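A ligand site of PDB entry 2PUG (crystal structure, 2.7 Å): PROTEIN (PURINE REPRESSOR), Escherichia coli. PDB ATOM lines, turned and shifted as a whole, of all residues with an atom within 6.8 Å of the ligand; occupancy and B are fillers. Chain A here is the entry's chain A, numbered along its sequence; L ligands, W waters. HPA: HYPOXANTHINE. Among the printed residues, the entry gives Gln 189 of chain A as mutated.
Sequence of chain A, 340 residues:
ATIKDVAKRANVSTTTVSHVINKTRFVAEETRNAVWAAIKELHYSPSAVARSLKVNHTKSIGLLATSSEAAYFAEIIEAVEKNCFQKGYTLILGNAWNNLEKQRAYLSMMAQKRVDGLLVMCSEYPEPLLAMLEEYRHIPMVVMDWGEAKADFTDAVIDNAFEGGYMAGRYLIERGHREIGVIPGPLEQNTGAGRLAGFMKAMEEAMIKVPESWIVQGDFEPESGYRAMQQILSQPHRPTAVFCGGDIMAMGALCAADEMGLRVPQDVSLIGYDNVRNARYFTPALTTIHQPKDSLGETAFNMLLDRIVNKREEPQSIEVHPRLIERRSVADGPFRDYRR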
ATOM      1  N   THR A  66     -30.354  22.126 -15.785  1.00  0.00           N
ATOM      2  CA  THR A  66     -29.708  23.314 -15.226  1.00  0.00           C
ATOM      3  C   THR A  66     -28.523  23.715 -16.113  1.00  0.00           C
ATOM      4  O   THR A  66     -28.388  24.872 -16.512  1.00  0.00           O
ATOM      5  CB  THR A  66     -29.163  23.035 -13.827  1.00  0.00           C
ATOM      6  OG1 THR A  66     -30.242  22.893 -12.900  1.00  0.00           O
ATOM      7  CG2 THR A  66     -28.263  24.154 -13.397  1.00  0.00           C
ATOM      8  N   ALA A  70     -21.090  20.517 -16.765  1.00  0.00           N
ATOM      9  CA  ALA A  70     -20.657  19.785 -15.571  1.00  0.00           C
ATOM     10  C   ALA A  70     -20.725  18.263 -15.686  1.00  0.00           C
ATOM     11  O   ALA A  70     -21.765  17.688 -16.079  1.00  0.00           O
ATOM     12  CB  ALA A  70     -21.403  20.263 -14.349  1.00  0.00           C
ATOM     13  N   ALA A  71     -19.614  17.639 -15.354  1.00  0.00           N
ATOM     14  CA  ALA A  71     -19.460  16.193 -15.396  1.00  0.00           C
ATOM     15  C   ALA A  71     -20.686  15.446 -14.924  1.00  0.00           C
ATOM     16  O   ALA A  71     -21.203  14.577 -15.621  1.00  0.00           O
ATOM     17  CB  ALA A  71     -18.215  15.756 -14.538  1.00  0.00           C
ATOM     18  N   TYR A  72     -21.076  15.753 -13.689  1.00  0.00           N
ATOM     19  CA  TYR A  72     -22.206  15.113 -13.035  1.00  0.00           C
ATOM     20  C   TYR A  72     -23.374  15.106 -14.022  1.00  0.00           C
ATOM     21  O   TYR A  72     -23.822  14.066 -14.478  1.00  0.00           O
ATOM     22  CB  TYR A  72     -22.529  15.892 -11.743  1.00  0.00           C
ATOM     23  CG  TYR A  72     -23.710  15.374 -10.974  1.00  0.00           C
ATOM     24  CD1 TYR A  72     -23.727  14.099 -10.478  1.00  0.00           C
ATOM     25  CD2 TYR A  72     -24.824  16.172 -10.769  1.00  0.00           C
ATOM     26  CE1 TYR A  72     -24.814  13.618  -9.776  1.00  0.00           C
ATOM     27  CE2 TYR A  72     -25.900  15.712 -10.062  1.00  0.00           C
ATOM     28  CZ  TYR A  72     -25.888  14.420  -9.578  1.00  0.00           C
ATOM     29  OH  TYR A  72     -26.958  13.927  -8.885  1.00  0.00           O
ATOM     30  N   PHE A  73     -23.782  16.301 -14.421  1.00  0.00           N
ATOM     31  CA  PHE A  73     -24.865  16.448 -15.333  1.00  0.00           C
ATOM     32  C   PHE A  73     -24.685  15.721 -16.635  1.00  0.00           C
ATOM     33  O   PHE A  73     -25.586  14.997 -17.100  1.00  0.00           O
ATOM     34  CB  PHE A  73     -25.091  17.915 -15.603  1.00  0.00           C
ATOM     35  CG  PHE A  73     -25.661  18.650 -14.435  1.00  0.00           C
ATOM     36  CD1 PHE A  73     -26.609  18.044 -13.633  1.00  0.00           C
ATOM     37  CD2 PHE A  73     -25.242  19.928 -14.123  1.00  0.00           C
ATOM     38  CE1 PHE A  73     -27.138  18.695 -12.558  1.00  0.00           C
ATOM     39  CE2 PHE A  73     -25.755  20.591 -13.034  1.00  0.00           C
ATOM     40  CZ  PHE A  73     -26.698  19.966 -12.242  1.00  0.00           C
ATOM     41  N   SER A 123     -32.036  21.674 -10.112  1.00  0.00           N
ATOM     42  CA  SER A 123     -31.214  21.916  -8.921  1.00  0.00           C
ATOM     43  C   SER A 123     -32.059  22.571  -7.855  1.00  0.00           C
ATOM     44  O   SER A 123     -32.613  21.899  -7.010  1.00  0.00           O
ATOM     45  CB  SER A 123     -30.028  22.820  -9.271  1.00  0.00           C
ATOM     46  OG  SER A 123     -29.250  22.254 -10.331  1.00  0.00           O
ATOM     47  N   ASP A 159     -32.498  10.048  -4.749  1.00  0.00           N
ATOM     48  CA  ASP A 159     -31.130   9.548  -4.560  1.00  0.00           C
ATOM     49  C   ASP A 159     -30.655   9.156  -3.161  1.00  0.00           C
ATOM     50  O   ASP A 159     -29.608   8.537  -3.045  1.00  0.00           O
ATOM     51  CB  ASP A 159     -30.137  10.511  -5.195  1.00  0.00           C
ATOM     52  CG  ASP A 159     -30.073  11.832  -4.469  1.00  0.00           C
ATOM     53  OD1 ASP A 159     -30.810  11.969  -3.461  1.00  0.00           O
ATOM     54  OD2 ASP A 159     -29.298  12.717  -4.904  1.00  0.00           O
ATOM     55  N   PRO A 186     -24.294  23.903  -2.676  1.00  0.00           N
ATOM     56  CA  PRO A 186     -25.378  24.842  -2.350  1.00  0.00           C
ATOM     57  C   PRO A 186     -26.475  24.231  -1.482  1.00  0.00           C
ATOM     58  O   PRO A 186     -26.998  23.160  -1.769  1.00  0.00           O
ATOM     59  CB  PRO A 186     -25.935  25.235  -3.715  1.00  0.00           C
ATOM     60  CG  PRO A 186     -24.843  24.888  -4.695  1.00  0.00           C
ATOM     61  CD  PRO A 186     -24.199  23.667  -4.129  1.00  0.00           C
ATOM     62  N   GLN A 189     -29.973  23.030  -2.813  1.00  0.00           N
ATOM     63  CA  GLN A 189     -30.104  21.782  -3.590  1.00  0.00           C
ATOM     64  C   GLN A 189     -30.185  20.615  -2.625  1.00  0.00           C
ATOM     65  O   GLN A 189     -29.862  20.728  -1.454  1.00  0.00           O
ATOM     66  CB  GLN A 189     -28.943  21.549  -4.570  1.00  0.00           C
ATOM     67  CG  GLN A 189     -28.447  22.759  -5.246  1.00  0.00           C
ATOM     68  CD  GLN A 189     -27.645  22.415  -6.462  1.00  0.00           C
ATOM     69  OE1 GLN A 189     -27.020  23.271  -7.057  1.00  0.00           O
ATOM     70  NE2 GLN A 189     -27.685  21.142  -6.845  1.00  0.00           N
ATOM     71  N   ASN A 190     -30.616  19.485  -3.157  1.00  0.00           N
ATOM     72  CA  ASN A 190     -30.742  18.280  -2.408  1.00  0.00           C
ATOM     73  C   ASN A 190     -29.345  17.743  -2.176  1.00  0.00           C
ATOM     74  O   ASN A 190     -28.949  17.500  -1.023  1.00  0.00           O
ATOM     75  CB  ASN A 190     -31.560  17.293  -3.208  1.00  0.00           C
ATOM     76  CG  ASN A 190     -31.619  15.979  -2.560  1.00  0.00           C
ATOM     77  OD1 ASN A 190     -32.001  15.860  -1.399  1.00  0.00           O
ATOM     78  ND2 ASN A 190     -31.171  14.951  -3.282  1.00  0.00           N
ATOM     79  N   THR A 191     -28.602  17.584  -3.273  1.00  0.00           N
ATOM     80  CA  THR A 191     -27.215  17.096  -3.243  1.00  0.00           C
ATOM     81  C   THR A 191     -26.332  18.035  -2.440  1.00  0.00           C
ATOM     82  O   THR A 191     -25.180  17.734  -2.163  1.00  0.00           O
ATOM     83  CB  THR A 191     -26.636  16.982  -4.654  1.00  0.00           C
ATOM     84  OG1 THR A 191     -26.722  18.259  -5.304  1.00  0.00           O
ATOM     85  CG2 THR A 191     -27.409  15.917  -5.481  1.00  0.00           C
ATOM     86  N   GLY A 192     -26.882  19.188  -2.081  1.00  0.00           N
ATOM     87  CA  GLY A 192     -26.176  20.152  -1.275  1.00  0.00           C
ATOM     88  C   GLY A 192     -26.570  19.863   0.160  1.00  0.00           C
ATOM     89  O   GLY A 192     -25.909  19.109   0.880  1.00  0.00           O
ATOM     90  N   ARG A 195     -26.791  16.122   1.532  1.00  0.00           N
ATOM     91  CA  ARG A 195     -25.566  15.367   1.683  1.00  0.00           C
ATOM     92  C   ARG A 195     -24.907  15.821   3.010  1.00  0.00           C
ATOM     93  O   ARG A 195     -24.436  15.005   3.813  1.00  0.00           O
ATOM     94  CB  ARG A 195     -24.640  15.575   0.447  1.00  0.00           C
ATOM     95  CG  ARG A 195     -25.003  14.677  -0.776  1.00  0.00           C
ATOM     96  CD  ARG A 195     -24.252  15.138  -2.074  1.00  0.00           C
ATOM     97  NE  ARG A 195     -24.690  14.388  -3.269  1.00  0.00           N
ATOM     98  CZ  ARG A 195     -24.060  14.416  -4.440  1.00  0.00           C
ATOM     99  NH1 ARG A 195     -22.958  15.143  -4.590  1.00  0.00           N
ATOM    100  NH2 ARG A 195     -24.531  13.729  -5.481  1.00  0.00           N
ATOM    101  N   ASP A 219     -19.820  25.406  -4.738  1.00  0.00           N
ATOM    102  CA  ASP A 219     -20.867  25.592  -5.737  1.00  0.00           C
ATOM    103  C   ASP A 219     -20.781  24.510  -6.776  1.00  0.00           C
ATOM    104  O   ASP A 219     -21.272  24.670  -7.885  1.00  0.00           O
ATOM    105  CB  ASP A 219     -20.772  26.979  -6.375  1.00  0.00           C
ATOM    106  CG  ASP A 219     -19.487  27.175  -7.168  1.00  0.00           C
ATOM    107  OD1 ASP A 219     -18.675  26.232  -7.310  1.00  0.00           O
ATOM    108  OD2 ASP A 219     -19.316  28.287  -7.704  1.00  0.00           O
ATOM    109  N   PHE A 220     -20.127  23.412  -6.412  1.00  0.00           N
ATOM    110  CA  PHE A 220     -19.882  22.240  -7.284  1.00  0.00           C
ATOM    111  C   PHE A 220     -18.809  22.488  -8.316  1.00  0.00           C
ATOM    112  O   PHE A 220     -18.337  21.564  -8.948  1.00  0.00           O
ATOM    113  CB  PHE A 220     -21.159  21.764  -7.963  1.00  0.00           C
ATOM    114  CG  PHE A 220     -22.087  21.032  -7.061  1.00  0.00           C
ATOM    115  CD1 PHE A 220     -21.735  19.811  -6.540  1.00  0.00           C
ATOM    116  CD2 PHE A 220     -23.315  21.581  -6.733  1.00  0.00           C
ATOM    117  CE1 PHE A 220     -22.582  19.136  -5.700  1.00  0.00           C
ATOM    118  CE2 PHE A 220     -24.160  20.915  -5.896  1.00  0.00           C
ATOM    119  CZ  PHE A 220     -23.795  19.688  -5.378  1.00  0.00           C
ATOM    120  N   GLU A 221     -18.424  23.741  -8.477  1.00  0.00           N
ATOM    121  CA  GLU A 221     -17.387  24.057  -9.443  1.00  0.00           C
ATOM    122  C   GLU A 221     -15.974  23.986  -8.814  1.00  0.00           C
ATOM    123  O   GLU A 221     -15.723  24.492  -7.717  1.00  0.00           O
ATOM    124  CB  GLU A 221     -17.662  25.405 -10.103  1.00  0.00           C
ATOM    125  CG  GLU A 221     -18.951  25.448 -10.911  1.00  0.00           C
ATOM    126  CD  GLU A 221     -18.734  25.215 -12.405  1.00  0.00           C
ATOM    127  OE1 GLU A 221     -18.521  24.052 -12.815  1.00  0.00           O
ATOM    128  OE2 GLU A 221     -18.808  26.208 -13.173  1.00  0.00           O
ATOM    129  N   GLY A 245     -18.411  17.857  -0.916  1.00  0.00           N
ATOM    130  CA  GLY A 245     -19.745  17.597  -1.510  1.00  0.00           C
ATOM    131  C   GLY A 245     -19.828  17.048  -2.953  1.00  0.00           C
ATOM    132  O   GLY A 245     -20.815  16.427  -3.323  1.00  0.00           O
ATOM    133  N   GLY A 246     -18.790  17.297  -3.762  1.00  0.00           N
ATOM    134  CA  GLY A 246     -18.779  16.829  -5.154  1.00  0.00           C
ATOM    135  C   GLY A 246     -17.357  16.536  -5.674  1.00  0.00           C
ATOM    136  O   GLY A 246     -16.404  17.248  -5.386  1.00  0.00           O
ATOM    137  N   ASP A 247     -17.237  15.489  -6.462  1.00  0.00           N
ATOM    138  CA  ASP A 247     -15.942  15.119  -6.999  1.00  0.00           C
ATOM    139  C   ASP A 247     -15.205  16.266  -7.709  1.00  0.00           C
ATOM    140  O   ASP A 247     -13.986  16.457  -7.578  1.00  0.00           O
ATOM    141  CB  ASP A 247     -16.104  13.942  -7.924  1.00  0.00           C
ATOM    142  CG  ASP A 247     -16.395  12.653  -7.170  1.00  0.00           C
ATOM    143  OD1 ASP A 247     -16.487  12.698  -5.918  1.00  0.00           O
ATOM    144  OD2 ASP A 247     -16.413  11.589  -7.836  1.00  0.00           O
ATOM    145  N   ILE A 248     -15.946  17.023  -8.489  1.00  0.00           N
ATOM    146  CA  ILE A 248     -15.315  18.086  -9.214  1.00  0.00           C
ATOM    147  C   ILE A 248     -14.771  19.188  -8.301  1.00  0.00           C
ATOM    148  O   ILE A 248     -13.702  19.709  -8.542  1.00  0.00           O
ATOM    149  CB  ILE A 248     -16.174  18.576 -10.333  1.00  0.00           C
ATOM    150  CG1 ILE A 248     -16.499  17.390 -11.264  1.00  0.00           C
ATOM    151  CG2 ILE A 248     -15.499  19.715 -11.059  1.00  0.00           C
ATOM    152  CD1 ILE A 248     -15.582  17.246 -12.407  1.00  0.00           C
ATOM    153  N   TYR A 273     -17.824  12.954  -3.408  1.00  0.00           N
ATOM    154  CA  TYR A 273     -19.161  12.486  -3.600  1.00  0.00           C
ATOM    155  C   TYR A 273     -19.577  12.727  -5.020  1.00  0.00           C
ATOM    156  O   TYR A 273     -19.555  13.885  -5.484  1.00  0.00           O
ATOM    157  CB  TYR A 273     -20.111  13.238  -2.689  1.00  0.00           C
ATOM    158  CG  TYR A 273     -21.430  12.520  -2.478  1.00  0.00           C
ATOM    159  CD1 TYR A 273     -22.194  12.095  -3.562  1.00  0.00           C
ATOM    160  CD2 TYR A 273     -21.892  12.247  -1.214  1.00  0.00           C
ATOM    161  CE1 TYR A 273     -23.387  11.433  -3.373  1.00  0.00           C
ATOM    162  CE2 TYR A 273     -23.071  11.575  -1.011  1.00  0.00           C
ATOM    163  CZ  TYR A 273     -23.808  11.170  -2.079  1.00  0.00           C
ATOM    164  OH  TYR A 273     -24.985  10.504  -1.839  1.00  0.00           O
ATOM    165  N   ASP A 274     -19.998  11.628  -5.676  1.00  0.00           N
ATOM    166  CA  ASP A 274     -20.516  11.576  -7.055  1.00  0.00           C
ATOM    167  C   ASP A 274     -19.959  10.386  -7.803  1.00  0.00           C
ATOM    168  O   ASP A 274     -20.681   9.649  -8.494  1.00  0.00           O
ATOM    169  CB  ASP A 274     -20.237  12.839  -7.851  1.00  0.00           C
ATOM    170  CG  ASP A 274     -21.314  13.916  -7.647  1.00  0.00           C
ATOM    171  OD1 ASP A 274     -22.302  13.658  -6.937  1.00  0.00           O
ATOM    172  OD2 ASP A 274     -21.143  15.019  -8.203  1.00  0.00           O
ATOM    173  N   GLN A 291     -22.809   7.787  -7.012  1.00  0.00           N
ATOM    174  CA  GLN A 291     -24.206   8.085  -7.277  1.00  0.00           C
ATOM    175  C   GLN A 291     -24.454   7.330  -8.548  1.00  0.00           C
ATOM    176  O   GLN A 291     -23.662   7.423  -9.497  1.00  0.00           O
ATOM    177  CB  GLN A 291     -24.399   9.579  -7.561  1.00  0.00           C
ATOM    178  CG  GLN A 291     -25.806   9.954  -8.117  1.00  0.00           C
ATOM    179  CD  GLN A 291     -26.739  10.588  -7.045  1.00  0.00           C
ATOM    180  OE1 GLN A 291     -27.107  11.748  -7.140  1.00  0.00           O
ATOM    181  NE2 GLN A 291     -27.096   9.822  -6.036  1.00  0.00           N
HETATM  182  N1  HPA L   1     -23.957  20.126  -9.801  1.00  0.00           N
HETATM  183  C2  HPA L   1     -22.731  19.529 -10.057  1.00  0.00           C
HETATM  184  N3  HPA L   1     -22.350  18.368  -9.536  1.00  0.00           N
HETATM  185  C4  HPA L   1     -23.292  17.852  -8.712  1.00  0.00           C
HETATM  186  C5  HPA L   1     -24.539  18.367  -8.397  1.00  0.00           C
HETATM  187  C6  HPA L   1     -24.946  19.592  -8.979  1.00  0.00           C
HETATM  188  O6  HPA L   1     -26.012  20.194  -8.825  1.00  0.00           O
HETATM  189  N7  HPA L   1     -25.210  17.519  -7.523  1.00  0.00           N
HETATM  190  C8  HPA L   1     -24.384  16.527  -7.339  1.00  0.00           C
HETATM  191  N9  HPA L   1     -23.215  16.652  -8.054  1.00  0.00           N
HETATM  192  O   HOH W   1     -19.967  17.678 -11.790  1.00  0.00           O
HETATM  193  O   HOH W   2     -26.514  23.156  -9.791  1.00  0.00           O
HETATM  194  O   HOH W   3     -27.926  17.636  -8.228  1.00  0.00           O
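Residues that only touch the ligand: Tyr 72 (3.1 Å), Phe 73 (3.5 Å), Arg 195 (3.4 Å) and Phe 220 (3.3 Å).
The nearest printed residue that does not touch the ligand is Ser 123 (4.1 Å).
The side-chain amide oxygen (OE1) of Gln 291 is in hydrogen-bond range of the side-chain hydroxyl (OH) of Tyr 72, 2.8 Å away.
NE2 of Gln 189 is in hydrogen-bond range of OG1 of Thr 191, 3.4 Å away.
O of Asp 274 is in hydrogen-bond range of N of Gln 291 (3.2 Å).
The guanidinium group of Arg 195 sits at hydrogen-bond distance from the backbone carbonyl oxygen of Gly 245, 2.8 Å away.
The side-chain carboxylate of Asp 274 lies within salt-bridge range of the guanidinium group of Arg 195 (2.7 Å).
Water W3 lies within hydrogen-bond range of N7 of the ligand (2.8 Å) and OG1 of Thr 191 (3.2 Å).
Water W2 lies within hydrogen-bond range of OE1 of Gln 189, OG of Ser 123 and O6 of the ligand.
Water W1 lies within hydrogen-bond range of N of Tyr 72 (2.9 Å) and N3 of the ligand (3.4 Å).
The side-chain carboxylate of Asp 274 lies within hydrogen-bond range of a nitrogen (N9) of the ligand (2.6 Å).
NE2 of Gln 189 is in hydrogen-bond range of O6 of the ligand (2.8 Å).
A nitrogen (N7) of the ligand lies within hydrogen-bond range of the side-chain hydroxyl (OG1) of Thr 191 (2.8 Å).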
